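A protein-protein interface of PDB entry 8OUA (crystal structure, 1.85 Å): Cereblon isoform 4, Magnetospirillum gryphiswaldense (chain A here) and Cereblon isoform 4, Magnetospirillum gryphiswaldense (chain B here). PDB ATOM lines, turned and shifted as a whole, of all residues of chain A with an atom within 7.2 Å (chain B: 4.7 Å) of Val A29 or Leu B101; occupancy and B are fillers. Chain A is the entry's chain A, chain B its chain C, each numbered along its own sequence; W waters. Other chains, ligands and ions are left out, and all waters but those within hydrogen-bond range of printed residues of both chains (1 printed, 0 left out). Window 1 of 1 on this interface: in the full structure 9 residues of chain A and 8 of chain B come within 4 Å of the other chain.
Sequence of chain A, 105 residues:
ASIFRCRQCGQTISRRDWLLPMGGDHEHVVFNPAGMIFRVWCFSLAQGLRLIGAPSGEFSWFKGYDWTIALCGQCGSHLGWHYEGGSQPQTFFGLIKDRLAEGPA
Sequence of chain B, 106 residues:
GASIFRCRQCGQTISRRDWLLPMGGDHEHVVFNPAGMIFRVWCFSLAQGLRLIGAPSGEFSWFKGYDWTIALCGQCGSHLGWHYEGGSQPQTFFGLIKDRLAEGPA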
ATOM      1  N   GLU A  27       3.892 -24.724  14.967  1.00  0.00           N
ATOM      2  CA  GLU A  27       3.009 -24.939  13.855  1.00  0.00           C
ATOM      3  C   GLU A  27       3.745 -24.866  12.540  1.00  0.00           C
ATOM      4  O   GLU A  27       4.411 -23.888  12.275  1.00  0.00           O
ATOM      5  CB  GLU A  27       1.906 -23.905  13.866  1.00  0.00           C
ATOM      6  CG  GLU A  27       1.007 -24.032  12.704  1.00  0.00           C
ATOM      7  CD  GLU A  27      -0.170 -23.065  12.837  1.00  0.00           C
ATOM      8  OE1 GLU A  27      -1.243 -23.465  13.335  1.00  0.00           O
ATOM      9  OE2 GLU A  27       0.012 -21.893  12.506  1.00  0.00           O
ATOM     10  N   HIS A  28       3.553 -25.869  11.686  1.00  0.00           N
ATOM     11  CA  HIS A  28       4.126 -25.878  10.359  1.00  0.00           C
ATOM     12  C   HIS A  28       3.057 -26.190   9.337  1.00  0.00           C
ATOM     13  O   HIS A  28       2.288 -27.131   9.513  1.00  0.00           O
ATOM     14  CB  HIS A  28       5.219 -26.938  10.329  1.00  0.00           C
ATOM     15  CG  HIS A  28       6.363 -26.603  11.206  1.00  0.00           C
ATOM     16  ND1 HIS A  28       7.603 -26.221  10.722  1.00  0.00           N
ATOM     17  CD2 HIS A  28       6.442 -26.549  12.552  1.00  0.00           C
ATOM     18  CE1 HIS A  28       8.408 -26.000  11.758  1.00  0.00           C
ATOM     19  NE2 HIS A  28       7.698 -26.145  12.876  1.00  0.00           N
ATOM     20  N   VAL A  29       3.005 -25.429   8.240  1.00  0.00           N
ATOM     21  CA  VAL A  29       1.966 -25.683   7.254  1.00  0.00           C
ATOM     22  C   VAL A  29       2.657 -26.294   6.055  1.00  0.00           C
ATOM     23  O   VAL A  29       3.625 -25.723   5.589  1.00  0.00           O
ATOM     24  CB  VAL A  29       1.134 -24.419   6.886  1.00  0.00           C
ATOM     25  CG1 VAL A  29       0.034 -24.725   5.890  1.00  0.00           C
ATOM     26  CG2 VAL A  29       0.584 -23.761   8.095  1.00  0.00           C
ATOM     27  N   VAL A  30       2.179 -27.462   5.570  1.00  0.00           N
ATOM     28  CA  VAL A  30       2.961 -28.297   4.678  1.00  0.00           C
ATOM     29  C   VAL A  30       2.017 -28.916   3.682  1.00  0.00           C
ATOM     30  O   VAL A  30       0.832 -28.969   3.971  1.00  0.00           O
ATOM     31  CB  VAL A  30       3.774 -29.368   5.475  1.00  0.00           C
ATOM     32  CG1 VAL A  30       4.832 -28.749   6.354  1.00  0.00           C
ATOM     33  CG2 VAL A  30       2.910 -30.201   6.359  1.00  0.00           C
ATOM     34  N   PHE A  31       2.519 -29.397   2.536  1.00  0.00           N
ATOM     35  CA  PHE A  31       1.749 -30.186   1.593  1.00  0.00           C
ATOM     36  C   PHE A  31       2.498 -31.433   1.181  1.00  0.00           C
ATOM     37  O   PHE A  31       3.716 -31.461   1.130  1.00  0.00           O
ATOM     38  CB  PHE A  31       1.323 -29.395   0.355  1.00  0.00           C
ATOM     39  CG  PHE A  31       2.379 -28.929  -0.579  1.00  0.00           C
ATOM     40  CD1 PHE A  31       3.114 -27.770  -0.334  1.00  0.00           C
ATOM     41  CD2 PHE A  31       2.571 -29.602  -1.783  1.00  0.00           C
ATOM     42  CE1 PHE A  31       4.036 -27.321  -1.278  1.00  0.00           C
ATOM     43  CE2 PHE A  31       3.468 -29.132  -2.725  1.00  0.00           C
ATOM     44  CZ  PHE A  31       4.194 -27.998  -2.472  1.00  0.00           C
ATOM     45  N   ILE A  37      -2.848 -30.109   1.914  1.00  0.00           N
ATOM     46  CA  ILE A  37      -2.236 -29.168   2.814  1.00  0.00           C
ATOM     47  C   ILE A  37      -2.631 -29.546   4.264  1.00  0.00           C
ATOM     48  O   ILE A  37      -3.741 -29.989   4.518  1.00  0.00           O
ATOM     49  CB  ILE A  37      -2.598 -27.724   2.459  1.00  0.00           C
ATOM     50  CG1 ILE A  37      -1.979 -27.337   1.106  1.00  0.00           C
ATOM     51  CG2 ILE A  37      -2.123 -26.762   3.505  1.00  0.00           C
ATOM     52  CD1 ILE A  37      -2.514 -26.019   0.543  1.00  0.00           C
ATOM     53  N   PHE A  38      -1.650 -29.551   5.160  1.00  0.00           N
ATOM     54  CA  PHE A  38      -1.856 -29.875   6.578  1.00  0.00           C
ATOM     55  C   PHE A  38      -1.267 -28.757   7.382  1.00  0.00           C
ATOM     56  O   PHE A  38      -0.156 -28.251   7.128  1.00  0.00           O
ATOM     57  CB  PHE A  38      -1.206 -31.209   6.971  1.00  0.00           C
ATOM     58  CG  PHE A  38      -1.595 -32.448   6.204  1.00  0.00           C
ATOM     59  CD1 PHE A  38      -2.748 -33.133   6.477  1.00  0.00           C
ATOM     60  CD2 PHE A  38      -0.870 -32.828   5.078  1.00  0.00           C
ATOM     61  CE1 PHE A  38      -3.067 -34.249   5.747  1.00  0.00           C
ATOM     62  CE2 PHE A  38      -1.237 -33.922   4.340  1.00  0.00           C
ATOM     63  CZ  PHE A  38      -2.272 -34.693   4.725  1.00  0.00           C
ATOM     64  N   ARG A  39      -2.018 -28.383   8.423  1.00  0.00           N
ATOM     65  CA  ARG A  39      -1.481 -27.596   9.483  1.00  0.00           C
ATOM     66  C   ARG A  39      -1.031 -28.552  10.605  1.00  0.00           C
ATOM     67  O   ARG A  39      -1.850 -29.152  11.244  1.00  0.00           O
ATOM     68  CB  ARG A  39      -2.586 -26.727  10.043  1.00  0.00           C
ATOM     69  CG  ARG A  39      -2.015 -25.656  10.943  1.00  0.00           C
ATOM     70  N   VAL A  40       0.265 -28.726  10.739  1.00  0.00           N
ATOM     71  CA  VAL A  40       0.861 -29.698  11.614  1.00  0.00           C
ATOM     72  C   VAL A  40       1.314 -28.948  12.871  1.00  0.00           C
ATOM     73  O   VAL A  40       1.965 -27.881  12.791  1.00  0.00           O
ATOM     74  CB  VAL A  40       2.024 -30.375  10.906  1.00  0.00           C
ATOM     75  CG1 VAL A  40       2.824 -31.232  11.861  1.00  0.00           C
ATOM     76  CG2 VAL A  40       1.603 -31.214   9.726  1.00  0.00           C
ATOM     77  N   TRP A  61       9.020 -33.581   5.536  1.00  0.00           N
ATOM     78  CA  TRP A  61       8.986 -32.173   5.788  1.00  0.00           C
ATOM     79  C   TRP A  61      10.093 -31.730   6.737  1.00  0.00           C
ATOM     80  O   TRP A  61      10.294 -30.559   6.904  1.00  0.00           O
ATOM     81  CB  TRP A  61       7.614 -31.690   6.305  1.00  0.00           C
ATOM     82  CG  TRP A  61       6.517 -31.964   5.330  1.00  0.00           C
ATOM     83  CD1 TRP A  61       6.475 -31.620   4.011  1.00  0.00           C
ATOM     84  CD2 TRP A  61       5.297 -32.650   5.612  1.00  0.00           C
ATOM     85  NE1 TRP A  61       5.316 -32.091   3.449  1.00  0.00           N
ATOM     86  CE2 TRP A  61       4.556 -32.682   4.421  1.00  0.00           C
ATOM     87  CE3 TRP A  61       4.766 -33.257   6.753  1.00  0.00           C
ATOM     88  CZ2 TRP A  61       3.315 -33.300   4.333  1.00  0.00           C
ATOM     89  CZ3 TRP A  61       3.530 -33.835   6.672  1.00  0.00           C
ATOM     90  CH2 TRP A  61       2.795 -33.875   5.475  1.00  0.00           C
ATOM     91  N   PHE B   5       7.411 -23.908  -2.752  1.00  0.00           N
ATOM     92  CA  PHE B   5       6.750 -23.053  -1.794  1.00  0.00           C
ATOM     93  C   PHE B   5       5.432 -22.562  -2.406  1.00  0.00           C
ATOM     94  O   PHE B   5       5.412 -21.975  -3.500  1.00  0.00           O
ATOM     95  CB  PHE B   5       7.587 -21.836  -1.387  1.00  0.00           C
ATOM     96  CG  PHE B   5       8.975 -22.187  -0.885  1.00  0.00           C
ATOM     97  CD1 PHE B   5       9.984 -22.511  -1.789  1.00  0.00           C
ATOM     98  CD2 PHE B   5       9.229 -22.341   0.483  1.00  0.00           C
ATOM     99  CE1 PHE B   5      11.226 -22.969  -1.359  1.00  0.00           C
ATOM    100  CE2 PHE B   5      10.477 -22.772   0.919  1.00  0.00           C
ATOM    101  CZ  PHE B   5      11.476 -23.079   0.001  1.00  0.00           C
ATOM    102  N   ARG B   6       4.380 -22.656  -1.598  1.00  0.00           N
ATOM    103  CA  ARG B   6       3.019 -22.312  -1.977  1.00  0.00           C
ATOM    104  C   ARG B   6       2.394 -21.399  -0.949  1.00  0.00           C
ATOM    105  O   ARG B   6       2.800 -21.394   0.192  1.00  0.00           O
ATOM    106  CB  ARG B   6       2.232 -23.615  -2.175  1.00  0.00           C
ATOM    107  N   CYS B   7       1.390 -20.629  -1.348  1.00  0.00           N
ATOM    108  CA  CYS B   7       0.548 -19.881  -0.437  1.00  0.00           C
ATOM    109  C   CYS B   7      -0.080 -20.814   0.594  1.00  0.00           C
ATOM    110  O   CYS B   7      -0.765 -21.733   0.181  1.00  0.00           O
ATOM    111  CB  CYS B   7      -0.555 -19.157  -1.213  1.00  0.00           C
ATOM    112  SG  CYS B   7      -1.687 -18.278  -0.145  1.00  0.00           S
ATOM    113  N   ARG B   8       0.088 -20.494   1.909  1.00  0.00           N
ATOM    114  CA  ARG B   8      -0.446 -21.265   3.044  1.00  0.00           C
ATOM    115  C   ARG B   8      -1.978 -21.359   2.956  1.00  0.00           C
ATOM    116  O   ARG B   8      -2.568 -22.356   3.368  1.00  0.00           O
ATOM    117  CB  ARG B   8       0.120 -20.578   4.326  1.00  0.00           C
ATOM    118  CG  ARG B   8      -0.593 -20.666   5.681  1.00  0.00           C
ATOM    119  N   ILE B  14       4.235 -20.383  -5.663  1.00  0.00           N
ATOM    120  CA  ILE B  14       4.882 -19.076  -5.578  1.00  0.00           C
ATOM    121  C   ILE B  14       6.356 -19.186  -5.973  1.00  0.00           C
ATOM    122  O   ILE B  14       6.830 -18.390  -6.821  1.00  0.00           O
ATOM    123  CB  ILE B  14       4.734 -18.472  -4.179  1.00  0.00           C
ATOM    124  CG1 ILE B  14       3.263 -18.333  -3.768  1.00  0.00           C
ATOM    125  CG2 ILE B  14       5.448 -17.128  -4.050  1.00  0.00           C
ATOM    126  CD1 ILE B  14       2.451 -17.332  -4.548  1.00  0.00           C
ATOM    127  N   PHE B  44      14.142 -14.710  -2.600  1.00  0.00           N
ATOM    128  CA  PHE B  44      14.112 -15.483  -3.843  1.00  0.00           C
ATOM    129  C   PHE B  44      14.478 -14.588  -5.015  1.00  0.00           C
ATOM    130  O   PHE B  44      14.077 -13.442  -5.026  1.00  0.00           O
ATOM    131  CB  PHE B  44      12.713 -16.040  -4.093  1.00  0.00           C
ATOM    132  CG  PHE B  44      12.238 -17.063  -3.105  1.00  0.00           C
ATOM    133  CD1 PHE B  44      11.600 -16.675  -1.935  1.00  0.00           C
ATOM    134  CD2 PHE B  44      12.442 -18.424  -3.342  1.00  0.00           C
ATOM    135  CE1 PHE B  44      11.205 -17.654  -1.033  1.00  0.00           C
ATOM    136  CE2 PHE B  44      12.043 -19.386  -2.435  1.00  0.00           C
ATOM    137  CZ  PHE B  44      11.403 -18.991  -1.282  1.00  0.00           C
ATOM    138  N   LEU B  80       1.823 -12.168   1.165  1.00  0.00           N
ATOM    139  CA  LEU B  80       2.871 -13.178   1.341  1.00  0.00           C
ATOM    140  C   LEU B  80       4.265 -12.593   1.580  1.00  0.00           C
ATOM    141  O   LEU B  80       5.217 -13.340   1.885  1.00  0.00           O
ATOM    142  CB  LEU B  80       2.941 -14.090   0.123  1.00  0.00           C
ATOM    143  CG  LEU B  80       1.643 -14.883  -0.137  1.00  0.00           C
ATOM    144  CD1 LEU B  80       1.849 -15.800  -1.301  1.00  0.00           C
ATOM    145  CD2 LEU B  80       1.184 -15.671   1.103  1.00  0.00           C
ATOM    146  N   LEU B  96       9.804 -13.119   1.034  1.00  0.00           N
ATOM    147  CA  LEU B  96       8.529 -13.722   1.390  1.00  0.00           C
ATOM    148  C   LEU B  96       8.585 -14.183   2.840  1.00  0.00           C
ATOM    149  O   LEU B  96       9.603 -14.776   3.262  1.00  0.00           O
ATOM    150  CB  LEU B  96       8.246 -14.896   0.428  1.00  0.00           C
ATOM    151  CG  LEU B  96       8.162 -14.503  -1.063  1.00  0.00           C
ATOM    152  CD1 LEU B  96       7.834 -15.716  -1.926  1.00  0.00           C
ATOM    153  CD2 LEU B  96       7.171 -13.349  -1.290  1.00  0.00           C
ATOM    154  N   ILE B  97       7.429 -14.043   3.501  1.00  0.00           N
ATOM    155  CA  ILE B  97       7.279 -14.422   4.902  1.00  0.00           C
ATOM    156  C   ILE B  97       7.164 -15.936   5.033  1.00  0.00           C
ATOM    157  O   ILE B  97       6.159 -16.502   4.587  1.00  0.00           O
ATOM    158  CB  ILE B  97       6.023 -13.752   5.495  1.00  0.00           C
ATOM    159  CG1 ILE B  97       6.015 -12.261   5.192  1.00  0.00           C
ATOM    160  CG2 ILE B  97       5.885 -14.072   6.992  1.00  0.00           C
ATOM    161  CD1 ILE B  97       4.683 -11.602   5.368  1.00  0.00           C
ATOM    162  N   LYS B  98       8.145 -16.578   5.710  1.00  0.00           N
ATOM    163  CA  LYS B  98       8.199 -18.032   5.847  1.00  0.00           C
ATOM    164  C   LYS B  98       6.864 -18.554   6.374  1.00  0.00           C
ATOM    165  O   LYS B  98       6.321 -19.527   5.834  1.00  0.00           O
ATOM    166  CB  LYS B  98       9.398 -18.496   6.709  1.00  0.00           C
ATOM    167  N   ASP B  99       6.283 -17.856   7.369  1.00  0.00           N
ATOM    168  CA  ASP B  99       5.112 -18.395   8.051  1.00  0.00           C
ATOM    169  C   ASP B  99       3.861 -18.260   7.170  1.00  0.00           C
ATOM    170  O   ASP B  99       2.796 -18.725   7.538  1.00  0.00           O
ATOM    171  CB  ASP B  99       4.929 -17.778   9.447  1.00  0.00           C
ATOM    172  N   ARG B 100       3.954 -17.605   6.017  1.00  0.00           N
ATOM    173  CA  ARG B 100       2.789 -17.488   5.150  1.00  0.00           C
ATOM    174  C   ARG B 100       2.853 -18.476   3.990  1.00  0.00           C
ATOM    175  O   ARG B 100       1.977 -18.476   3.135  1.00  0.00           O
ATOM    176  CB  ARG B 100       2.697 -16.047   4.663  1.00  0.00           C
ATOM    177  CG  ARG B 100       2.548 -15.123   5.848  1.00  0.00           C
ATOM    178  CD  ARG B 100       1.376 -14.198   5.723  1.00  0.00           C
ATOM    179  NE  ARG B 100       1.181 -13.400   6.924  1.00  0.00           N
ATOM    180  CZ  ARG B 100       1.041 -12.081   6.946  1.00  0.00           C
ATOM    181  NH1 ARG B 100       1.131 -11.388   5.829  1.00  0.00           N
ATOM    182  NH2 ARG B 100       0.789 -11.460   8.087  1.00  0.00           N
ATOM    183  N   LEU B 101       3.900 -19.295   3.960  1.00  0.00           N
ATOM    184  CA  LEU B 101       4.080 -20.271   2.911  1.00  0.00           C
ATOM    185  C   LEU B 101       3.874 -21.667   3.474  1.00  0.00           C
ATOM    186  O   LEU B 101       4.038 -21.882   4.680  1.00  0.00           O
ATOM    187  CB  LEU B 101       5.502 -20.132   2.374  1.00  0.00           C
ATOM    188  CG  LEU B 101       5.836 -18.802   1.704  1.00  0.00           C
ATOM    189  CD1 LEU B 101       7.268 -18.832   1.151  1.00  0.00           C
ATOM    190  CD2 LEU B 101       4.869 -18.477   0.559  1.00  0.00           C
ATOM    191  N   ALA B 102       3.515 -22.590   2.566  1.00  0.00           N
ATOM    192  CA  ALA B 102       3.561 -24.016   2.799  1.00  0.00           C
ATOM    193  C   ALA B 102       4.674 -24.577   1.922  1.00  0.00           C
ATOM    194  O   ALA B 102       4.868 -24.122   0.773  1.00  0.00           O
ATOM    195  CB  ALA B 102       2.206 -24.633   2.509  1.00  0.00           C
ATOM    196  N   GLU B 103       5.397 -25.557   2.472  1.00  0.00           N
ATOM    197  CA  GLU B 103       6.495 -26.181   1.723  1.00  0.00           C
ATOM    198  C   GLU B 103       6.088 -27.617   1.413  1.00  0.00           C
ATOM    199  O   GLU B 103       5.327 -28.254   2.166  1.00  0.00           O
ATOM    200  CB  GLU B 103       7.822 -26.063   2.486  1.00  0.00           C
HETATM  201  O   HOH W   1       5.708 -23.088   6.293  1.00  0.00           O
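The backbone NH (N) of Phe A31 is in hydrogen-bond range of the backbone carbonyl oxygen (O) of Glu B103, at 3.1 Å.
The backbone carbonyl oxygen of Val A30 is in hydrogen-bond range of the backbone NH of Phe A38, at 2.8 Å. The backbone carbonyl oxygen (O) of Phe A31 sits at hydrogen-bond distance from the indole nitrogen (NE1) of Trp A61. The backbone carbonyl oxygen (O) of Arg B6 lies within hydrogen-bond range of the backbone NH (N) of Ala B102 (2.8 Å).
Among the printed residues, pairs that only touch across the chains: Val A29 with Ala B102 (3.3 Å), Val A30 with Glu B103 (3.5 Å), Val A29 with Glu B103 (3.6 Å), Phe A31 with Ala B102 (3.9 Å) and Val A29 with Leu B101 (3.97 Å).
Of chain B, only Leu B101 (3.97 Å), Ala B102 (3.3 Å) and Glu B103 (3.6 Å) come within 4 Å of Val A29. Of chain A, only Val A29 comes within 4 Å of Leu B101. Of the printed residues of chain B, Val A30 touches Glu B103 (3.5 Å). Of the printed residues of chain B, Phe A31 touches Ala B102 (3.9 Å) and Glu B103 (3.1 Å). Ile A37 touches none of the printed residues of chain B. The nearest residue of chain A that does not touch Leu B101 is Val A30 (5.9 Å). The nearest printed residue of chain A that does not touch Ala B102 is Val A30 (4.2 Å).
Hydrophobic or aromatic side chains of chain A within 4 Å of the printed part of chain B: Val A30 and Phe A31. Of the 15 printed residues of chain B, 3 touch a printed residue of chain A. Along chain B the printed residues that touch a printed residue of chain A span positions 101 to 103. Among the printed residues, no Asp or Glu carboxylate lies within 4 Å of a Lys or Arg side-chain nitrogen of the other chain.
Water W1 lies within hydrogen-bond range of O of Leu B101 (2.6 Å) and O of Val A29 (3.4 Å).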
